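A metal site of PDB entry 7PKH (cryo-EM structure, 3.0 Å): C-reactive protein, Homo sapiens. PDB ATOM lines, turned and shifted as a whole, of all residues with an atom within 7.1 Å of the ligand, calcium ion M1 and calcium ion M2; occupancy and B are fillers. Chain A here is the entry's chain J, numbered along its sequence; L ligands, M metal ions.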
ATOM      1  N   TYR A  49      -5.725  24.947 -11.831  1.00  0.00           N
ATOM      2  CA  TYR A  49      -6.016  24.555 -13.194  1.00  0.00           C
ATOM      3  C   TYR A  49      -5.648  25.682 -14.151  1.00  0.00           C
ATOM      4  O   TYR A  49      -5.744  26.854 -13.805  1.00  0.00           O
ATOM      5  CB  TYR A  49      -7.482  24.151 -13.323  1.00  0.00           C
ATOM      6  CG  TYR A  49      -8.410  25.245 -12.882  1.00  0.00           C
ATOM      7  CD1 TYR A  49      -8.791  25.340 -11.563  1.00  0.00           C
ATOM      8  CD2 TYR A  49      -8.887  26.185 -13.767  1.00  0.00           C
ATOM      9  CE1 TYR A  49      -9.634  26.317 -11.135  1.00  0.00           C
ATOM     10  CE2 TYR A  49      -9.728  27.186 -13.343  1.00  0.00           C
ATOM     11  CZ  TYR A  49     -10.096  27.242 -12.028  1.00  0.00           C
ATOM     12  OH  TYR A  49     -10.922  28.230 -11.575  1.00  0.00           O
ATOM     13  N   SER A  50      -5.232  25.304 -15.359  1.00  0.00           N
ATOM     14  CA  SER A  50      -4.981  26.271 -16.423  1.00  0.00           C
ATOM     15  C   SER A  50      -6.256  26.764 -17.085  1.00  0.00           C
ATOM     16  O   SER A  50      -7.078  25.968 -17.551  1.00  0.00           O
ATOM     17  CB  SER A  50      -4.081  25.644 -17.472  1.00  0.00           C
ATOM     18  OG  SER A  50      -3.913  26.516 -18.572  1.00  0.00           O
ATOM     19  N   SER A  53      -3.559  29.125 -21.969  1.00  0.00           N
ATOM     20  CA  SER A  53      -2.125  28.844 -22.042  1.00  0.00           C
ATOM     21  C   SER A  53      -1.597  29.119 -23.446  1.00  0.00           C
ATOM     22  O   SER A  53      -1.827  28.349 -24.378  1.00  0.00           O
ATOM     23  CB  SER A  53      -1.842  27.404 -21.648  1.00  0.00           C
ATOM     24  OG  SER A  53      -0.461  27.220 -21.399  1.00  0.00           O
ATOM     25  N   ALA A  55       1.737  29.510 -25.632  1.00  0.00           N
ATOM     26  CA  ALA A  55       3.130  29.077 -25.608  1.00  0.00           C
ATOM     27  C   ALA A  55       3.850  29.422 -26.894  1.00  0.00           C
ATOM     28  O   ALA A  55       3.264  29.473 -27.974  1.00  0.00           O
ATOM     29  CB  ALA A  55       3.217  27.578 -25.374  1.00  0.00           C
ATOM     30  N   GLN A  59       9.367  29.599 -25.024  1.00  0.00           N
ATOM     31  CA  GLN A  59       8.802  29.941 -23.723  1.00  0.00           C
ATOM     32  C   GLN A  59       7.410  29.334 -23.633  1.00  0.00           C
ATOM     33  O   GLN A  59       6.493  29.750 -24.343  1.00  0.00           O
ATOM     34  CB  GLN A  59       8.741  31.455 -23.557  1.00  0.00           C
ATOM     35  CG  GLN A  59       8.110  31.906 -22.256  1.00  0.00           C
ATOM     36  CD  GLN A  59       8.705  31.228 -21.072  1.00  0.00           C
ATOM     37  OE1 GLN A  59       8.143  30.277 -20.537  1.00  0.00           O
ATOM     38  NE2 GLN A  59       9.864  31.697 -20.647  1.00  0.00           N
ATOM     39  N   ASP A  60       7.256  28.343 -22.755  1.00  0.00           N
ATOM     40  CA  ASP A  60       5.998  27.610 -22.638  1.00  0.00           C
ATOM     41  C   ASP A  60       4.924  28.377 -21.870  1.00  0.00           C
ATOM     42  O   ASP A  60       3.751  28.032 -21.978  1.00  0.00           O
ATOM     43  CB  ASP A  60       6.236  26.254 -21.965  1.00  0.00           C
ATOM     44  CG  ASP A  60       6.711  26.382 -20.537  1.00  0.00           C
ATOM     45  OD1 ASP A  60       7.764  27.015 -20.332  1.00  0.00           O
ATOM     46  OD2 ASP A  60       6.050  25.844 -19.636  1.00  0.00           O
ATOM     47  N   ASN A  61       5.308  29.396 -21.095  1.00  0.00           N
ATOM     48  CA  ASN A  61       4.347  30.219 -20.385  1.00  0.00           C
ATOM     49  C   ASN A  61       4.410  31.634 -20.929  1.00  0.00           C
ATOM     50  O   ASN A  61       4.605  32.597 -20.183  1.00  0.00           O
ATOM     51  CB  ASN A  61       4.619  30.230 -18.881  1.00  0.00           C
ATOM     52  CG  ASN A  61       4.461  28.876 -18.260  1.00  0.00           C
ATOM     53  OD1 ASN A  61       4.255  27.876 -18.955  1.00  0.00           O
ATOM     54  ND2 ASN A  61       4.535  28.823 -16.937  1.00  0.00           N
ATOM     55  N   LEU A  64       0.103  32.903 -19.668  1.00  0.00           N
ATOM     56  CA  LEU A  64      -0.683  31.910 -18.964  1.00  0.00           C
ATOM     57  C   LEU A  64      -1.564  32.589 -17.942  1.00  0.00           C
ATOM     58  O   LEU A  64      -1.077  33.383 -17.127  1.00  0.00           O
ATOM     59  CB  LEU A  64       0.222  30.859 -18.311  1.00  0.00           C
ATOM     60  CG  LEU A  64      -0.385  29.836 -17.360  1.00  0.00           C
ATOM     61  CD1 LEU A  64      -1.168  28.798 -18.112  1.00  0.00           C
ATOM     62  CD2 LEU A  64       0.709  29.187 -16.567  1.00  0.00           C
ATOM     63  N   PHE A  66      -3.736  31.348 -14.867  1.00  0.00           N
ATOM     64  CA  PHE A  66      -3.797  30.147 -14.042  1.00  0.00           C
ATOM     65  C   PHE A  66      -4.468  30.462 -12.728  1.00  0.00           C
ATOM     66  O   PHE A  66      -4.135  31.441 -12.071  1.00  0.00           O
ATOM     67  CB  PHE A  66      -2.386  29.598 -13.802  1.00  0.00           C
ATOM     68  CG  PHE A  66      -2.355  28.179 -13.370  1.00  0.00           C
ATOM     69  CD1 PHE A  66      -2.216  27.168 -14.285  1.00  0.00           C
ATOM     70  CD2 PHE A  66      -2.442  27.852 -12.030  1.00  0.00           C
ATOM     71  CE1 PHE A  66      -2.169  25.860 -13.879  1.00  0.00           C
ATOM     72  CE2 PHE A  66      -2.407  26.543 -11.633  1.00  0.00           C
ATOM     73  CZ  PHE A  66      -2.279  25.554 -12.546  1.00  0.00           C
ATOM     74  N   TRP A  67      -5.437  29.630 -12.354  1.00  0.00           N
ATOM     75  CA  TRP A  67      -5.960  29.613 -10.994  1.00  0.00           C
ATOM     76  C   TRP A  67      -5.092  28.742 -10.113  1.00  0.00           C
ATOM     77  O   TRP A  67      -4.886  27.568 -10.417  1.00  0.00           O
ATOM     78  CB  TRP A  67      -7.401  29.100 -10.962  1.00  0.00           C
ATOM     79  CG  TRP A  67      -7.932  29.069  -9.591  1.00  0.00           C
ATOM     80  CD1 TRP A  67      -7.878  28.041  -8.717  1.00  0.00           C
ATOM     81  CD2 TRP A  67      -8.518  30.163  -8.874  1.00  0.00           C
ATOM     82  NE1 TRP A  67      -8.436  28.386  -7.529  1.00  0.00           N
ATOM     83  CE2 TRP A  67      -8.838  29.695  -7.595  1.00  0.00           C
ATOM     84  CE3 TRP A  67      -8.817  31.475  -9.194  1.00  0.00           C
ATOM     85  CZ2 TRP A  67      -9.438  30.491  -6.646  1.00  0.00           C
ATOM     86  CZ3 TRP A  67      -9.404  32.273  -8.251  1.00  0.00           C
ATOM     87  CH2 TRP A  67      -9.718  31.773  -6.989  1.00  0.00           C
ATOM     88  N   SER A  68      -4.594  29.305  -9.019  1.00  0.00           N
ATOM     89  CA  SER A  68      -3.777  28.577  -8.067  1.00  0.00           C
ATOM     90  C   SER A  68      -4.515  28.455  -6.746  1.00  0.00           C
ATOM     91  O   SER A  68      -4.983  29.460  -6.193  1.00  0.00           O
ATOM     92  CB  SER A  68      -2.428  29.274  -7.870  1.00  0.00           C
ATOM     93  OG  SER A  68      -2.615  30.599  -7.436  1.00  0.00           O
ATOM     94  N   SER A  74      -3.269  33.512 -11.087  1.00  0.00           N
ATOM     95  CA  SER A  74      -1.898  33.761 -11.492  1.00  0.00           C
ATOM     96  C   SER A  74      -1.886  34.237 -12.928  1.00  0.00           C
ATOM     97  O   SER A  74      -2.401  33.554 -13.817  1.00  0.00           O
ATOM     98  CB  SER A  74      -1.069  32.490 -11.336  1.00  0.00           C
ATOM     99  OG  SER A  74       0.175  32.611 -11.989  1.00  0.00           O
ATOM    100  N   PHE A  75      -1.326  35.416 -13.167  1.00  0.00           N
ATOM    101  CA  PHE A  75      -1.086  35.921 -14.508  1.00  0.00           C
ATOM    102  C   PHE A  75       0.413  35.979 -14.745  1.00  0.00           C
ATOM    103  O   PHE A  75       1.130  36.665 -14.004  1.00  0.00           O
ATOM    104  CB  PHE A  75      -1.705  37.301 -14.712  1.00  0.00           C
ATOM    105  CG  PHE A  75      -1.711  37.745 -16.147  1.00  0.00           C
ATOM    106  CD1 PHE A  75      -2.516  37.134 -17.067  1.00  0.00           C
ATOM    107  CD2 PHE A  75      -0.889  38.763 -16.571  1.00  0.00           C
ATOM    108  CE1 PHE A  75      -2.507  37.530 -18.377  1.00  0.00           C
ATOM    109  CE2 PHE A  75      -0.880  39.159 -17.881  1.00  0.00           C
ATOM    110  CZ  PHE A  75      -1.691  38.539 -18.782  1.00  0.00           C
ATOM    111  N   THR A  76       0.883  35.256 -15.749  1.00  0.00           N
ATOM    112  CA  THR A  76       2.293  35.286 -16.100  1.00  0.00           C
ATOM    113  C   THR A  76       2.470  35.496 -17.588  1.00  0.00           C
ATOM    114  O   THR A  76       1.757  34.914 -18.408  1.00  0.00           O
ATOM    115  CB  THR A  76       2.977  33.979 -15.692  1.00  0.00           C
ATOM    116  OG1 THR A  76       4.342  34.006 -16.114  1.00  0.00           O
ATOM    117  CG2 THR A  76       2.317  32.799 -16.305  1.00  0.00           C
ATOM    118  N   GLU A  81       5.560  36.205 -13.198  1.00  0.00           N
ATOM    119  CA  GLU A  81       4.215  35.949 -12.697  1.00  0.00           C
ATOM    120  C   GLU A  81       3.830  37.036 -11.707  1.00  0.00           C
ATOM    121  O   GLU A  81       4.636  37.473 -10.896  1.00  0.00           O
ATOM    122  CB  GLU A  81       4.156  34.594 -12.008  1.00  0.00           C
ATOM    123  CG  GLU A  81       2.827  34.227 -11.405  1.00  0.00           C
ATOM    124  CD  GLU A  81       2.925  33.034 -10.475  1.00  0.00           C
ATOM    125  OE1 GLU A  81       4.042  32.715 -10.023  1.00  0.00           O
ATOM    126  OE2 GLU A  81       1.878  32.430 -10.173  1.00  0.00           O
ATOM    127  N   LEU A  83       0.218  37.866  -9.089  1.00  0.00           N
ATOM    128  CA  LEU A  83      -1.012  37.278  -8.583  1.00  0.00           C
ATOM    129  C   LEU A  83      -2.041  38.363  -8.278  1.00  0.00           C
ATOM    130  O   LEU A  83      -1.686  39.451  -7.820  1.00  0.00           O
ATOM    131  CB  LEU A  83      -0.734  36.462  -7.325  1.00  0.00           C
ATOM    132  CG  LEU A  83       0.038  35.176  -7.644  1.00  0.00           C
ATOM    133  CD1 LEU A  83       1.522  35.234  -8.047  1.00  0.00           C
ATOM    134  CD2 LEU A  83      -0.459  33.811  -7.207  1.00  0.00           C
ATOM    135  N   GLU A 138      -2.537  22.863 -19.387  1.00  0.00           N
ATOM    136  CA  GLU A 138      -1.320  23.643 -19.302  1.00  0.00           C
ATOM    137  C   GLU A 138      -0.259  22.933 -20.115  1.00  0.00           C
ATOM    138  O   GLU A 138      -0.134  21.702 -20.027  1.00  0.00           O
ATOM    139  CB  GLU A 138      -0.907  23.806 -17.840  1.00  0.00           C
ATOM    140  CG  GLU A 138      -0.075  25.029 -17.504  1.00  0.00           C
ATOM    141  CD  GLU A 138       1.253  25.069 -18.229  1.00  0.00           C
ATOM    142  OE1 GLU A 138       1.928  24.021 -18.291  1.00  0.00           O
ATOM    143  OE2 GLU A 138       1.635  26.154 -18.709  1.00  0.00           O
ATOM    144  N   GLN A 139       0.485  23.674 -20.914  1.00  0.00           N
ATOM    145  CA  GLN A 139       1.486  23.080 -21.783  1.00  0.00           C
ATOM    146  C   GLN A 139       2.885  23.565 -21.429  1.00  0.00           C
ATOM    147  O   GLN A 139       3.075  24.704 -20.990  1.00  0.00           O
ATOM    148  CB  GLN A 139       1.171  23.370 -23.245  1.00  0.00           C
ATOM    149  CG  GLN A 139       1.073  24.818 -23.603  1.00  0.00           C
ATOM    150  CD  GLN A 139       0.728  25.013 -25.045  1.00  0.00           C
ATOM    151  OE1 GLN A 139       1.024  24.172 -25.884  1.00  0.00           O
ATOM    152  NE2 GLN A 139       0.108  26.131 -25.363  1.00  0.00           N
ATOM    153  N   ASP A 140       3.863  22.688 -21.620  1.00  0.00           N
ATOM    154  CA  ASP A 140       5.239  22.906 -21.210  1.00  0.00           C
ATOM    155  C   ASP A 140       6.231  22.757 -22.337  1.00  0.00           C
ATOM    156  O   ASP A 140       7.303  23.351 -22.271  1.00  0.00           O
ATOM    157  CB  ASP A 140       5.628  21.950 -20.079  1.00  0.00           C
ATOM    158  CG  ASP A 140       4.833  22.179 -18.819  1.00  0.00           C
ATOM    159  OD1 ASP A 140       4.189  21.218 -18.338  1.00  0.00           O
ATOM    160  OD2 ASP A 140       4.836  23.315 -18.309  1.00  0.00           O
ATOM    161  N   SER A 141       5.902  22.006 -23.386  1.00  0.00           N
ATOM    162  CA  SER A 141       6.512  22.167 -24.680  1.00  0.00           C
ATOM    163  C   SER A 141       5.585  22.991 -25.574  1.00  0.00           C
ATOM    164  O   SER A 141       4.572  23.509 -25.119  1.00  0.00           O
ATOM    165  CB  SER A 141       6.822  20.803 -25.299  1.00  0.00           C
ATOM    166  OG  SER A 141       5.643  20.044 -25.471  1.00  0.00           O
ATOM    167  N   GLY A 144       2.332  20.316 -25.800  1.00  0.00           N
ATOM    168  CA  GLY A 144       2.203  19.066 -25.083  1.00  0.00           C
ATOM    169  C   GLY A 144       2.952  19.079 -23.775  1.00  0.00           C
ATOM    170  O   GLY A 144       3.252  20.137 -23.220  1.00  0.00           O
ATOM    171  N   ASN A 145       3.258  17.878 -23.297  1.00  0.00           N
ATOM    172  CA  ASN A 145       3.682  17.676 -21.911  1.00  0.00           C
ATOM    173  C   ASN A 145       2.620  18.168 -20.934  1.00  0.00           C
ATOM    174  O   ASN A 145       2.917  18.815 -19.931  1.00  0.00           O
ATOM    175  CB  ASN A 145       5.029  18.353 -21.652  1.00  0.00           C
ATOM    176  CG  ASN A 145       6.145  17.764 -22.485  1.00  0.00           C
ATOM    177  OD1 ASN A 145       6.175  17.911 -23.704  1.00  0.00           O
ATOM    178  ND2 ASN A 145       7.074  17.092 -21.836  1.00  0.00           N
ATOM    179  N   PHE A 146       1.364  17.885 -21.252  1.00  0.00           N
ATOM    180  CA  PHE A 146       0.251  18.292 -20.413  1.00  0.00           C
ATOM    181  C   PHE A 146       0.294  17.553 -19.071  1.00  0.00           C
ATOM    182  O   PHE A 146       0.781  16.422 -18.986  1.00  0.00           O
ATOM    183  CB  PHE A 146      -1.073  18.022 -21.111  1.00  0.00           C
ATOM    184  CG  PHE A 146      -1.149  18.591 -22.494  1.00  0.00           C
ATOM    185  CD1 PHE A 146      -0.967  19.935 -22.712  1.00  0.00           C
ATOM    186  CD2 PHE A 146      -1.409  17.776 -23.573  1.00  0.00           C
ATOM    187  CE1 PHE A 146      -1.051  20.459 -23.965  1.00  0.00           C
ATOM    188  CE2 PHE A 146      -1.490  18.302 -24.841  1.00  0.00           C
ATOM    189  CZ  PHE A 146      -1.312  19.642 -25.030  1.00  0.00           C
ATOM    190  N   GLU A 147      -0.214  18.210 -18.037  1.00  0.00           N
ATOM    191  CA  GLU A 147      -0.255  17.653 -16.687  1.00  0.00           C
ATOM    192  C   GLU A 147      -1.703  17.558 -16.234  1.00  0.00           C
ATOM    193  O   GLU A 147      -2.411  18.564 -16.196  1.00  0.00           O
ATOM    194  CB  GLU A 147       0.561  18.518 -15.725  1.00  0.00           C
ATOM    195  CG  GLU A 147       1.925  18.911 -16.270  1.00  0.00           C
ATOM    196  CD  GLU A 147       2.796  19.570 -15.228  1.00  0.00           C
ATOM    197  OE1 GLU A 147       3.514  20.529 -15.571  1.00  0.00           O
ATOM    198  OE2 GLU A 147       2.758  19.128 -14.063  1.00  0.00           O
ATOM    199  N   GLN A 150      -3.161  19.894 -13.729  1.00  0.00           N
ATOM    200  CA  GLN A 150      -3.352  21.269 -14.172  1.00  0.00           C
ATOM    201  C   GLN A 150      -4.467  21.421 -15.191  1.00  0.00           C
ATOM    202  O   GLN A 150      -4.745  22.554 -15.611  1.00  0.00           O
ATOM    203  CB  GLN A 150      -2.037  21.799 -14.740  1.00  0.00           C
ATOM    204  CG  GLN A 150      -0.919  21.801 -13.721  1.00  0.00           C
ATOM    205  CD  GLN A 150       0.358  22.435 -14.223  1.00  0.00           C
ATOM    206  OE1 GLN A 150       0.722  22.302 -15.376  1.00  0.00           O
ATOM    207  NE2 GLN A 150       1.041  23.134 -13.334  1.00  0.00           N
HETATM  208  P1  LIG L   1       4.097  25.144 -15.050  1.00  0.00           P
HETATM  209  O1  LIG L   1       3.581  23.627 -15.073  1.00  0.00           O
HETATM  210  O2  LIG L   1       5.462  25.186 -14.500  1.00  0.00           O
HETATM  211  O3  LIG L   1       4.049  25.714 -16.552  1.00  0.00           O
HETATM  212  O4  LIG L   1       3.099  25.982 -14.105  1.00  0.00           O
HETATM  213  C1  LIG L   1       3.836  27.122 -13.661  1.00  0.00           C
HETATM  214  C2  LIG L   1       2.902  28.300 -13.346  1.00  0.00           C
HETATM  215  N1  LIG L   1       1.933  28.110 -12.255  1.00  0.00           N
HETATM  216  C3  LIG L   1       2.599  27.586 -11.056  1.00  0.00           C
HETATM  217  C4  LIG L   1       0.885  27.177 -12.650  1.00  0.00           C
HETATM  218  C5  LIG L   1       1.347  29.407 -11.913  1.00  0.00           C
HETATM  219 CA    CA M   1       3.904  25.463 -18.762  1.00  0.00          CA
HETATM  220 CA    CA M   2       2.768  22.440 -16.738  1.00  0.00          CA
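The side-chain carboxylate (OD1) of Asp 60 lies close to the side-chain amide oxygen (OE1) of Gln 59, 3.3 Å away. OE1 of Gln 59 sits at hydrogen-bond distance from N of Asn 61, at 3.0 Å. The backbone NH (N) of Ser 50 is in hydrogen-bond range of the backbone carbonyl oxygen (O) of Gln 150 (2.8 Å). The side-chain amide nitrogen of Gln 139 is in hydrogen-bond range of the backbone carbonyl oxygen of Ser 53, 3.1 Å away. O of Phe 66 is in hydrogen-bond range of N of Ser 74 (2.5 Å). The side-chain hydroxyl (OG) of Ser 74 sits at hydrogen-bond distance from the side-chain carboxylate (OE2) of Glu 81, 2.5 Å away. N of Leu 64 lies within hydrogen-bond range of O of Thr 76 (2.9 Å).
CD2 of Leu 64 touches C2 of the ligand (3.996 Å). Phe 66 touches the ligand. Ser 74 touches the ligand (OG to C5, 3.4 Å). OE2 of Glu 81 touches C5 of the ligand (3.5 Å). Hydrophobic or aromatic side chains within 4 Å of the ligand: Leu 64 and Phe 66. Within 4 Å of the ligand: Asp 60, Asn 61, Leu 64, Phe 66, Ser 74, Glu 81, Glu 138, Asp 140, Glu 147 and Gln 150. The nearest printed residue that does not touch the ligand is Gln 139 (4.7 Å).
Four residues have an atom within 4 Å of calcium ion M2: Glu 138, Asp 140, Glu 147 and Gln 150. The nearest printed residue that does not touch calcium ion M2 is Gln 139 (4.8 Å).
Calcium ion M1 is bound by O3 of the ligand (2.2 Å). OD2 of Asp 60 binds calcium ion M1, at 2.3 Å. The side-chain carboxylate (OE2) of Glu 138 binds calcium ion M1. Calcium ion M1 is bound by the side-chain carboxylate (OD2) of Asp 140 (2.4 Å). OD1 of Asn 61 binds calcium ion M1 (2.4 Å). OE1 of Glu 138 binds calcium ion M1 (2.5 Å). O of Gln 139 is bound to calcium ion M1 (2.5 Å).
O1 of the ligand binds calcium ion M2 (2.2 Å). OE1 of Glu 147 binds calcium ion M2 (2.4 Å). Calcium ion M2 is bound by OE1 of Glu 138 (2.4 Å). OE1 of Gln 150 binds calcium ion M2 (2.5 Å). The side-chain carboxylate (OD1) of Asp 140 is bound to calcium ion M2, at 2.5 Å. Calcium ion M2 is bound by OD2 of Asp 140 (2.7 Å).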
